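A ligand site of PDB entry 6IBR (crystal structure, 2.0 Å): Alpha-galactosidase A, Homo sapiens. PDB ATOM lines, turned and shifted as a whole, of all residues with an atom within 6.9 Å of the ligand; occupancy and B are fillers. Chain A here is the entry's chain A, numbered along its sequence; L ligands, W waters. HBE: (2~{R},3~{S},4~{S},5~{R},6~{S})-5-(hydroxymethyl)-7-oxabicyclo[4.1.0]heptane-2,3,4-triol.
A carbon (C2) of the ligand is covalently linked to the side-chain carboxylate (OD2) of Asp 139.
The side-chain carboxylate (OD1) of Asp 61 is in hydrogen-bond range of an oxygen (O7) of the ligand (2.5 Å).
OD2 of Asp 62 is in hydrogen-bond range of O11 of the ligand.
OE1 of Glu 172 sits at hydrogen-bond distance from O9 of the ligand, 2.7 Å away.
O9 of the ligand is in hydrogen-bond range of OD1 of Asp 200, at 2.7 Å.
O8 of the ligand sits at hydrogen-bond distance from NZ of Lys 137 (2.8 Å).
An oxygen (O8) of the ligand lies within hydrogen-bond range of the guanidinium group (NH1) of Arg 196, at 3.2 Å.
OD2 of Asp 139 is in hydrogen-bond range of OH of Tyr 103, 3.0 Å away.
OD1 of Asp 139 sits at hydrogen-bond distance from OH of Tyr 176.
OD2 of Asp 61 lies within salt-bridge range of NZ of Lys 137 (2.6 Å).
The side-chain carboxylate of Asp 62 sits at hydrogen-bond distance from the side-chain hydroxyl of Thr 110.
The guanidinium group (NH1) of Arg 196 is in salt-bridge range of the side-chain carboxylate (OE1) of Glu 172, 3.4 Å away.
The backbone carbonyl oxygen (O) of Arg 196 lies within hydrogen-bond range of the backbone NH (N) of Leu 175 (3.1 Å).
SG of Cys 111 forms a disulfide with SG of Cys 141 (2.1 Å).
The side-chain sulfur of Cys 63 is disulfide-bonded to the side-chain sulfur of Cys 21, at 2.0 Å.
CH2 of Trp 16 touches O11 of the ligand (3.6 Å).
Tyr 103 touches the ligand.
Cys 111 touches the ligand.
Hydrophobic or aromatic side chains within 4 Å of the ligand: Trp 16 and Tyr 103.
Within 4 Å of the ligand: Trp 16, Asp 61, Asp 62, Tyr 103, Cys 111, Lys 137, Asp 139, Glu 172, Arg 196 and Asp 200.
The nearest printed residue that does not touch the ligand is Ala 112 (4.1 Å).
Water W1 bridges the side-chain carboxylate (OD2) of Asp 235 (2.6 Å) and an oxygen (O8) of the ligand (2.6 Å).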
ATOM      1  N   LEU A  14       8.497  -6.908   5.816  1.00  0.00           N
ATOM      2  CA  LEU A  14       9.624  -7.703   5.250  1.00  0.00           C
ATOM      3  C   LEU A  14       9.311  -9.182   5.479  1.00  0.00           C
ATOM      4  O   LEU A  14       8.965  -9.544   6.611  1.00  0.00           O
ATOM      5  CB  LEU A  14      10.881  -7.233   5.987  1.00  0.00           C
ATOM      6  CG  LEU A  14      12.201  -7.783   5.483  1.00  0.00           C
ATOM      7  CD1 LEU A  14      12.403  -7.471   4.007  1.00  0.00           C
ATOM      8  CD2 LEU A  14      13.339  -7.197   6.296  1.00  0.00           C
ATOM      9  N   TRP A  16      11.052 -11.947   5.763  1.00  0.00           N
ATOM     10  CA  TRP A  16      12.065 -12.960   6.150  1.00  0.00           C
ATOM     11  C   TRP A  16      11.669 -13.771   7.399  1.00  0.00           C
ATOM     12  O   TRP A  16      11.693 -15.005   7.314  1.00  0.00           O
ATOM     13  CB  TRP A  16      13.431 -12.368   6.414  1.00  0.00           C
ATOM     14  CG  TRP A  16      14.433 -13.445   6.666  1.00  0.00           C
ATOM     15  CD1 TRP A  16      15.113 -13.707   7.823  1.00  0.00           C
ATOM     16  CD2 TRP A  16      14.858 -14.433   5.716  1.00  0.00           C
ATOM     17  NE1 TRP A  16      15.941 -14.782   7.649  1.00  0.00           N
ATOM     18  CE2 TRP A  16      15.802 -15.246   6.369  1.00  0.00           C
ATOM     19  CE3 TRP A  16      14.520 -14.717   4.396  1.00  0.00           C
ATOM     20  CZ2 TRP A  16      16.421 -16.327   5.722  1.00  0.00           C
ATOM     21  CZ3 TRP A  16      15.130 -15.781   3.765  1.00  0.00           C
ATOM     22  CH2 TRP A  16      16.077 -16.562   4.422  1.00  0.00           C
ATOM     23  N   CYS A  21      12.811 -18.810   3.608  1.00  0.00           N
ATOM     24  CA  CYS A  21      13.208 -19.235   2.238  1.00  0.00           C
ATOM     25  C   CYS A  21      12.323 -20.393   1.782  1.00  0.00           C
ATOM     26  O   CYS A  21      12.873 -21.369   1.255  1.00  0.00           O
ATOM     27  CB  CYS A  21      14.681 -19.627   2.184  1.00  0.00           C
ATOM     28  SG  CYS A  21      15.338 -19.711   0.494  1.00  0.00           S
ATOM     29  N   ASP A  61      12.807 -10.089   0.830  1.00  0.00           N
ATOM     30  CA  ASP A  61      14.103 -10.490   1.450  1.00  0.00           C
ATOM     31  C   ASP A  61      14.697 -11.562   0.535  1.00  0.00           C
ATOM     32  O   ASP A  61      14.320 -11.598  -0.649  1.00  0.00           O
ATOM     33  CB  ASP A  61      13.935 -10.934   2.911  1.00  0.00           C
ATOM     34  CG  ASP A  61      15.158 -10.728   3.781  1.00  0.00           C
ATOM     35  OD1 ASP A  61      16.040 -11.611   3.766  1.00  0.00           O
ATOM     36  OD2 ASP A  61      15.242  -9.669   4.482  1.00  0.00           O
ATOM     37  N   ASP A  62      15.576 -12.400   1.064  1.00  0.00           N
ATOM     38  CA  ASP A  62      16.316 -13.423   0.274  1.00  0.00           C
ATOM     39  C   ASP A  62      15.299 -14.383  -0.369  1.00  0.00           C
ATOM     40  O   ASP A  62      14.107 -14.417   0.069  1.00  0.00           O
ATOM     41  CB  ASP A  62      17.345 -14.108   1.179  1.00  0.00           C
ATOM     42  CG  ASP A  62      18.520 -14.739   0.462  1.00  0.00           C
ATOM     43  OD1 ASP A  62      18.470 -14.862  -0.788  1.00  0.00           O
ATOM     44  OD2 ASP A  62      19.478 -15.091   1.165  1.00  0.00           O
ATOM     45  N   CYS A  63      15.747 -15.096  -1.404  1.00  0.00           N
ATOM     46  CA  CYS A  63      15.061 -16.225  -2.106  1.00  0.00           C
ATOM     47  C   CYS A  63      13.982 -15.736  -3.084  1.00  0.00           C
ATOM     48  O   CYS A  63      13.046 -16.484  -3.336  1.00  0.00           O
ATOM     49  CB  CYS A  63      14.524 -17.247  -1.103  1.00  0.00           C
ATOM     50  SG  CYS A  63      15.798 -17.796   0.077  1.00  0.00           S
ATOM     51  N   TYR A 103      16.154  -7.319  -2.080  1.00  0.00           N
ATOM     52  CA  TYR A 103      17.316  -7.829  -1.319  1.00  0.00           C
ATOM     53  C   TYR A 103      18.411  -8.243  -2.320  1.00  0.00           C
ATOM     54  O   TYR A 103      18.040  -8.702  -3.410  1.00  0.00           O
ATOM     55  CB  TYR A 103      16.866  -9.002  -0.454  1.00  0.00           C
ATOM     56  CG  TYR A 103      17.951  -9.845   0.184  1.00  0.00           C
ATOM     57  CD1 TYR A 103      18.621 -10.802  -0.541  1.00  0.00           C
ATOM     58  CD2 TYR A 103      18.220  -9.770   1.544  1.00  0.00           C
ATOM     59  CE1 TYR A 103      19.584 -11.599   0.039  1.00  0.00           C
ATOM     60  CE2 TYR A 103      19.171 -10.580   2.146  1.00  0.00           C
ATOM     61  CZ  TYR A 103      19.861 -11.495   1.385  1.00  0.00           C
ATOM     62  OH  TYR A 103      20.816 -12.301   1.944  1.00  0.00           O
ATOM     63  N   ASP A 105      23.135  -9.221  -1.874  1.00  0.00           N
ATOM     64  CA  ASP A 105      24.236  -9.543  -0.926  1.00  0.00           C
ATOM     65  C   ASP A 105      25.537  -8.958  -1.511  1.00  0.00           C
ATOM     66  O   ASP A 105      25.771  -9.089  -2.719  1.00  0.00           O
ATOM     67  CB  ASP A 105      24.270 -11.049  -0.626  1.00  0.00           C
ATOM     68  CG  ASP A 105      25.273 -11.444   0.441  1.00  0.00           C
ATOM     69  OD1 ASP A 105      26.508 -11.347   0.177  1.00  0.00           O
ATOM     70  OD2 ASP A 105      24.825 -11.847   1.539  1.00  0.00           O
ATOM     71  N   THR A 110      24.141 -14.824  -1.975  1.00  0.00           N
ATOM     72  CA  THR A 110      23.246 -14.425  -0.865  1.00  0.00           C
ATOM     73  C   THR A 110      23.428 -15.438   0.261  1.00  0.00           C
ATOM     74  O   THR A 110      24.029 -16.503   0.014  1.00  0.00           O
ATOM     75  CB  THR A 110      21.806 -14.275  -1.348  1.00  0.00           C
ATOM     76  OG1 THR A 110      21.196 -15.564  -1.454  1.00  0.00           O
ATOM     77  CG2 THR A 110      21.728 -13.529  -2.665  1.00  0.00           C
ATOM     78  N   CYS A 111      22.937 -15.150   1.462  1.00  0.00           N
ATOM     79  CA  CYS A 111      23.100 -16.072   2.606  1.00  0.00           C
ATOM     80  C   CYS A 111      22.444 -17.417   2.271  1.00  0.00           C
ATOM     81  O   CYS A 111      22.968 -18.439   2.720  1.00  0.00           O
ATOM     82  CB  CYS A 111      22.564 -15.478   3.909  1.00  0.00           C
ATOM     83  SG  CYS A 111      23.455 -13.971   4.375  1.00  0.00           S
ATOM     84  N   ALA A 112      21.362 -17.429   1.473  1.00  0.00           N
ATOM     85  CA  ALA A 112      20.604 -18.663   1.155  1.00  0.00           C
ATOM     86  C   ALA A 112      21.154 -19.328  -0.120  1.00  0.00           C
ATOM     87  O   ALA A 112      20.635 -20.376  -0.499  1.00  0.00           O
ATOM     88  CB  ALA A 112      19.133 -18.335   1.035  1.00  0.00           C
ATOM     89  N   GLY A 113      22.168 -18.758  -0.774  1.00  0.00           N
ATOM     90  CA  GLY A 113      22.969 -19.442  -1.812  1.00  0.00           C
ATOM     91  C   GLY A 113      22.671 -18.976  -3.232  1.00  0.00           C
ATOM     92  O   GLY A 113      23.228 -19.588  -4.161  1.00  0.00           O
ATOM     93  N   LYS A 137      17.827  -3.854   0.729  1.00  0.00           N
ATOM     94  CA  LYS A 137      18.502  -4.475   1.899  1.00  0.00           C
ATOM     95  C   LYS A 137      19.654  -5.304   1.346  1.00  0.00           C
ATOM     96  O   LYS A 137      19.403  -6.165   0.493  1.00  0.00           O
ATOM     97  CB  LYS A 137      17.513  -5.314   2.711  1.00  0.00           C
ATOM     98  CG  LYS A 137      18.152  -6.151   3.805  1.00  0.00           C
ATOM     99  CD  LYS A 137      17.201  -7.054   4.513  1.00  0.00           C
ATOM    100  CE  LYS A 137      17.891  -7.986   5.482  1.00  0.00           C
ATOM    101  NZ  LYS A 137      16.901  -8.734   6.295  1.00  0.00           N
ATOM    102  N   ASP A 139      22.675  -7.744   2.289  1.00  0.00           N
ATOM    103  CA  ASP A 139      23.222  -8.675   3.309  1.00  0.00           C
ATOM    104  C   ASP A 139      24.716  -8.894   3.055  1.00  0.00           C
ATOM    105  O   ASP A 139      25.185  -8.535   1.971  1.00  0.00           O
ATOM    106  CB  ASP A 139      22.396  -9.954   3.310  1.00  0.00           C
ATOM    107  CG  ASP A 139      22.234 -10.593   4.668  1.00  0.00           C
ATOM    108  OD1 ASP A 139      23.065 -10.363   5.532  1.00  0.00           O
ATOM    109  OD2 ASP A 139      21.109 -11.471   4.842  1.00  0.00           O
ATOM    110  N   GLY A 140      25.446  -9.461   4.026  1.00  0.00           N
ATOM    111  CA  GLY A 140      26.919  -9.480   4.069  1.00  0.00           C
ATOM    112  C   GLY A 140      27.557 -10.871   3.932  1.00  0.00           C
ATOM    113  O   GLY A 140      28.769 -10.978   4.220  1.00  0.00           O
ATOM    114  N   CYS A 141      26.811 -11.896   3.499  1.00  0.00           N
ATOM    115  CA  CYS A 141      27.335 -13.298   3.444  1.00  0.00           C
ATOM    116  C   CYS A 141      28.308 -13.461   2.269  1.00  0.00           C
ATOM    117  O   CYS A 141      28.225 -12.679   1.277  1.00  0.00           O
ATOM    118  CB  CYS A 141      26.230 -14.338   3.344  1.00  0.00           C
ATOM    119  SG  CYS A 141      25.341 -14.657   4.892  1.00  0.00           S
ATOM    120  N   GLU A 172      24.218  -4.116   6.143  1.00  0.00           N
ATOM    121  CA  GLU A 172      24.547  -5.026   7.258  1.00  0.00           C
ATOM    122  C   GLU A 172      26.062  -4.989   7.507  1.00  0.00           C
ATOM    123  O   GLU A 172      26.598  -5.934   8.110  1.00  0.00           O
ATOM    124  CB  GLU A 172      23.999  -6.421   6.978  1.00  0.00           C
ATOM    125  CG  GLU A 172      22.520  -6.426   6.667  1.00  0.00           C
ATOM    126  CD  GLU A 172      21.812  -7.731   6.909  1.00  0.00           C
ATOM    127  OE1 GLU A 172      22.023  -8.346   7.976  1.00  0.00           O
ATOM    128  OE2 GLU A 172      21.062  -8.156   6.000  1.00  0.00           O
ATOM    129  N   LEU A 175      27.334  -5.391  11.354  1.00  0.00           N
ATOM    130  CA  LEU A 175      27.094  -6.801  11.751  1.00  0.00           C
ATOM    131  C   LEU A 175      28.238  -7.699  11.263  1.00  0.00           C
ATOM    132  O   LEU A 175      28.736  -8.467  12.071  1.00  0.00           O
ATOM    133  CB  LEU A 175      25.767  -7.278  11.146  1.00  0.00           C
ATOM    134  CG  LEU A 175      25.439  -8.746  11.401  1.00  0.00           C
ATOM    135  CD1 LEU A 175      25.489  -9.051  12.900  1.00  0.00           C
ATOM    136  CD2 LEU A 175      24.086  -9.106  10.807  1.00  0.00           C
ATOM    137  N   TYR A 176      28.613  -7.617   9.978  1.00  0.00           N
ATOM    138  CA  TYR A 176      29.563  -8.565   9.333  1.00  0.00           C
ATOM    139  C   TYR A 176      31.022  -8.189   9.623  1.00  0.00           C
ATOM    140  O   TYR A 176      31.909  -9.045   9.456  1.00  0.00           O
ATOM    141  CB  TYR A 176      29.258  -8.703   7.842  1.00  0.00           C
ATOM    142  CG  TYR A 176      28.103  -9.648   7.648  1.00  0.00           C
ATOM    143  CD1 TYR A 176      28.309 -11.012   7.557  1.00  0.00           C
ATOM    144  CD2 TYR A 176      26.807  -9.188   7.726  1.00  0.00           C
ATOM    145  CE1 TYR A 176      27.242 -11.893   7.441  1.00  0.00           C
ATOM    146  CE2 TYR A 176      25.731 -10.043   7.602  1.00  0.00           C
ATOM    147  CZ  TYR A 176      25.942 -11.402   7.470  1.00  0.00           C
ATOM    148  OH  TYR A 176      24.880 -12.230   7.344  1.00  0.00           O
ATOM    149  N   ARG A 196      22.277  -2.871  10.085  1.00  0.00           N
ATOM    150  CA  ARG A 196      22.073  -3.996  11.015  1.00  0.00           C
ATOM    151  C   ARG A 196      23.342  -4.096  11.888  1.00  0.00           C
ATOM    152  O   ARG A 196      24.483  -4.136  11.351  1.00  0.00           O
ATOM    153  CB  ARG A 196      21.710  -5.248  10.201  1.00  0.00           C
ATOM    154  CG  ARG A 196      20.235  -5.302   9.766  1.00  0.00           C
ATOM    155  CD  ARG A 196      19.291  -5.737  10.877  1.00  0.00           C
ATOM    156  NE  ARG A 196      19.834  -6.946  11.486  1.00  0.00           N
ATOM    157  CZ  ARG A 196      19.807  -8.158  10.915  1.00  0.00           C
ATOM    158  NH1 ARG A 196      19.154  -8.373   9.773  1.00  0.00           N
ATOM    159  NH2 ARG A 196      20.431  -9.160  11.517  1.00  0.00           N
ATOM    160  N   PHE A 198      23.387  -6.454  14.696  1.00  0.00           N
ATOM    161  CA  PHE A 198      23.315  -7.681  15.530  1.00  0.00           C
ATOM    162  C   PHE A 198      22.634  -8.828  14.782  1.00  0.00           C
ATOM    163  O   PHE A 198      21.990  -8.608  13.736  1.00  0.00           O
ATOM    164  CB  PHE A 198      22.617  -7.374  16.860  1.00  0.00           C
ATOM    165  CG  PHE A 198      22.803  -8.404  17.949  1.00  0.00           C
ATOM    166  CD1 PHE A 198      24.052  -8.577  18.561  1.00  0.00           C
ATOM    167  CD2 PHE A 198      21.754  -9.193  18.381  1.00  0.00           C
ATOM    168  CE1 PHE A 198      24.229  -9.508  19.574  1.00  0.00           C
ATOM    169  CE2 PHE A 198      21.939 -10.142  19.379  1.00  0.00           C
ATOM    170  CZ  PHE A 198      23.171 -10.284  19.981  1.00  0.00           C
ATOM    171  N   ALA A 199      22.832 -10.034  15.315  1.00  0.00           N
ATOM    172  CA  ALA A 199      22.373 -11.343  14.785  1.00  0.00           C
ATOM    173  C   ALA A 199      20.873 -11.282  14.455  1.00  0.00           C
ATOM    174  O   ALA A 199      20.120 -10.569  15.142  1.00  0.00           O
ATOM    175  CB  ALA A 199      22.674 -12.431  15.786  1.00  0.00           C
ATOM    176  N   ASP A 200      20.489 -11.981  13.403  1.00  0.00           N
ATOM    177  CA  ASP A 200      19.081 -12.129  12.939  1.00  0.00           C
ATOM    178  C   ASP A 200      18.163 -12.390  14.124  1.00  0.00           C
ATOM    179  O   ASP A 200      18.469 -13.234  14.979  1.00  0.00           O
ATOM    180  CB  ASP A 200      18.974 -13.243  11.901  1.00  0.00           C
ATOM    181  CG  ASP A 200      19.819 -13.007  10.654  1.00  0.00           C
ATOM    182  OD1 ASP A 200      20.493 -11.953  10.563  1.00  0.00           O
ATOM    183  OD2 ASP A 200      19.783 -13.892   9.780  1.00  0.00           O
ATOM    184  N   ILE A 201      17.079 -11.631  14.216  1.00  0.00           N
ATOM    185  CA  ILE A 201      16.022 -11.849  15.214  1.00  0.00           C
ATOM    186  C   ILE A 201      15.322 -13.182  14.888  1.00  0.00           C
ATOM    187  O   ILE A 201      15.278 -13.576  13.677  1.00  0.00           O
ATOM    188  CB  ILE A 201      15.062 -10.654  15.228  1.00  0.00           C
ATOM    189  CG1 ILE A 201      14.257 -10.656  16.528  1.00  0.00           C
ATOM    190  CG2 ILE A 201      14.183 -10.650  13.969  1.00  0.00           C
ATOM    191  CD1 ILE A 201      13.407  -9.420  16.725  1.00  0.00           C
ATOM    192  N   ASP A 235      16.596  -5.038  13.810  1.00  0.00           N
ATOM    193  CA  ASP A 235      15.915  -6.109  13.035  1.00  0.00           C
ATOM    194  C   ASP A 235      14.388  -6.023  13.258  1.00  0.00           C
ATOM    195  O   ASP A 235      13.905  -5.098  13.968  1.00  0.00           O
ATOM    196  CB  ASP A 235      16.520  -7.473  13.324  1.00  0.00           C
ATOM    197  CG  ASP A 235      16.461  -8.455  12.163  1.00  0.00           C
ATOM    198  OD1 ASP A 235      15.854  -8.083  11.124  1.00  0.00           O
ATOM    199  OD2 ASP A 235      16.989  -9.579  12.301  1.00  0.00           O
ATOM    200  N   MET A 236      13.666  -6.954  12.642  1.00  0.00           N
ATOM    201  CA  MET A 236      12.211  -6.911  12.368  1.00  0.00           C
ATOM    202  C   MET A 236      11.408  -6.970  13.681  1.00  0.00           C
ATOM    203  O   MET A 236      11.872  -7.588  14.678  1.00  0.00           O
ATOM    204  CB  MET A 236      11.804  -8.060  11.450  1.00  0.00           C
ATOM    205  CG  MET A 236      12.449  -7.994  10.059  1.00  0.00           C
ATOM    206  SD  MET A 236      12.416  -9.585   9.181  1.00  0.00           S
ATOM    207  CE  MET A 236      13.958 -10.314   9.727  1.00  0.00           C
HETATM  208  C3  HBE L   1      20.122 -11.096   7.024  1.00  0.00           C
HETATM  209  C4  HBE L   1      18.783 -11.700   7.448  1.00  0.00           C
HETATM  210  C5  HBE L   1      18.123 -12.240   6.197  1.00  0.00           C
HETATM  211  C1  HBE L   1      20.411 -13.397   5.941  1.00  0.00           C
HETATM  212  C2  HBE L   1      20.996 -12.006   6.135  1.00  0.00           C
HETATM  213  C6  HBE L   1      18.911 -13.452   5.688  1.00  0.00           C
HETATM  214  O7  HBE L   1      18.054 -11.194   5.203  1.00  0.00           O
HETATM  215  O8  HBE L   1      17.930 -10.711   8.001  1.00  0.00           O
HETATM  216  O9  HBE L   1      20.835 -10.707   8.173  1.00  0.00           O
HETATM  217  C10 HBE L   1      18.599 -13.665   4.212  1.00  0.00           C
HETATM  218  O11 HBE L   1      19.202 -14.866   3.755  1.00  0.00           O
HETATM  219  O12 HBE L   1      20.790 -14.029   7.143  1.00  0.00           O
HETATM  220  O   HOH W   1      16.905 -11.364  10.355  1.00  0.00           O
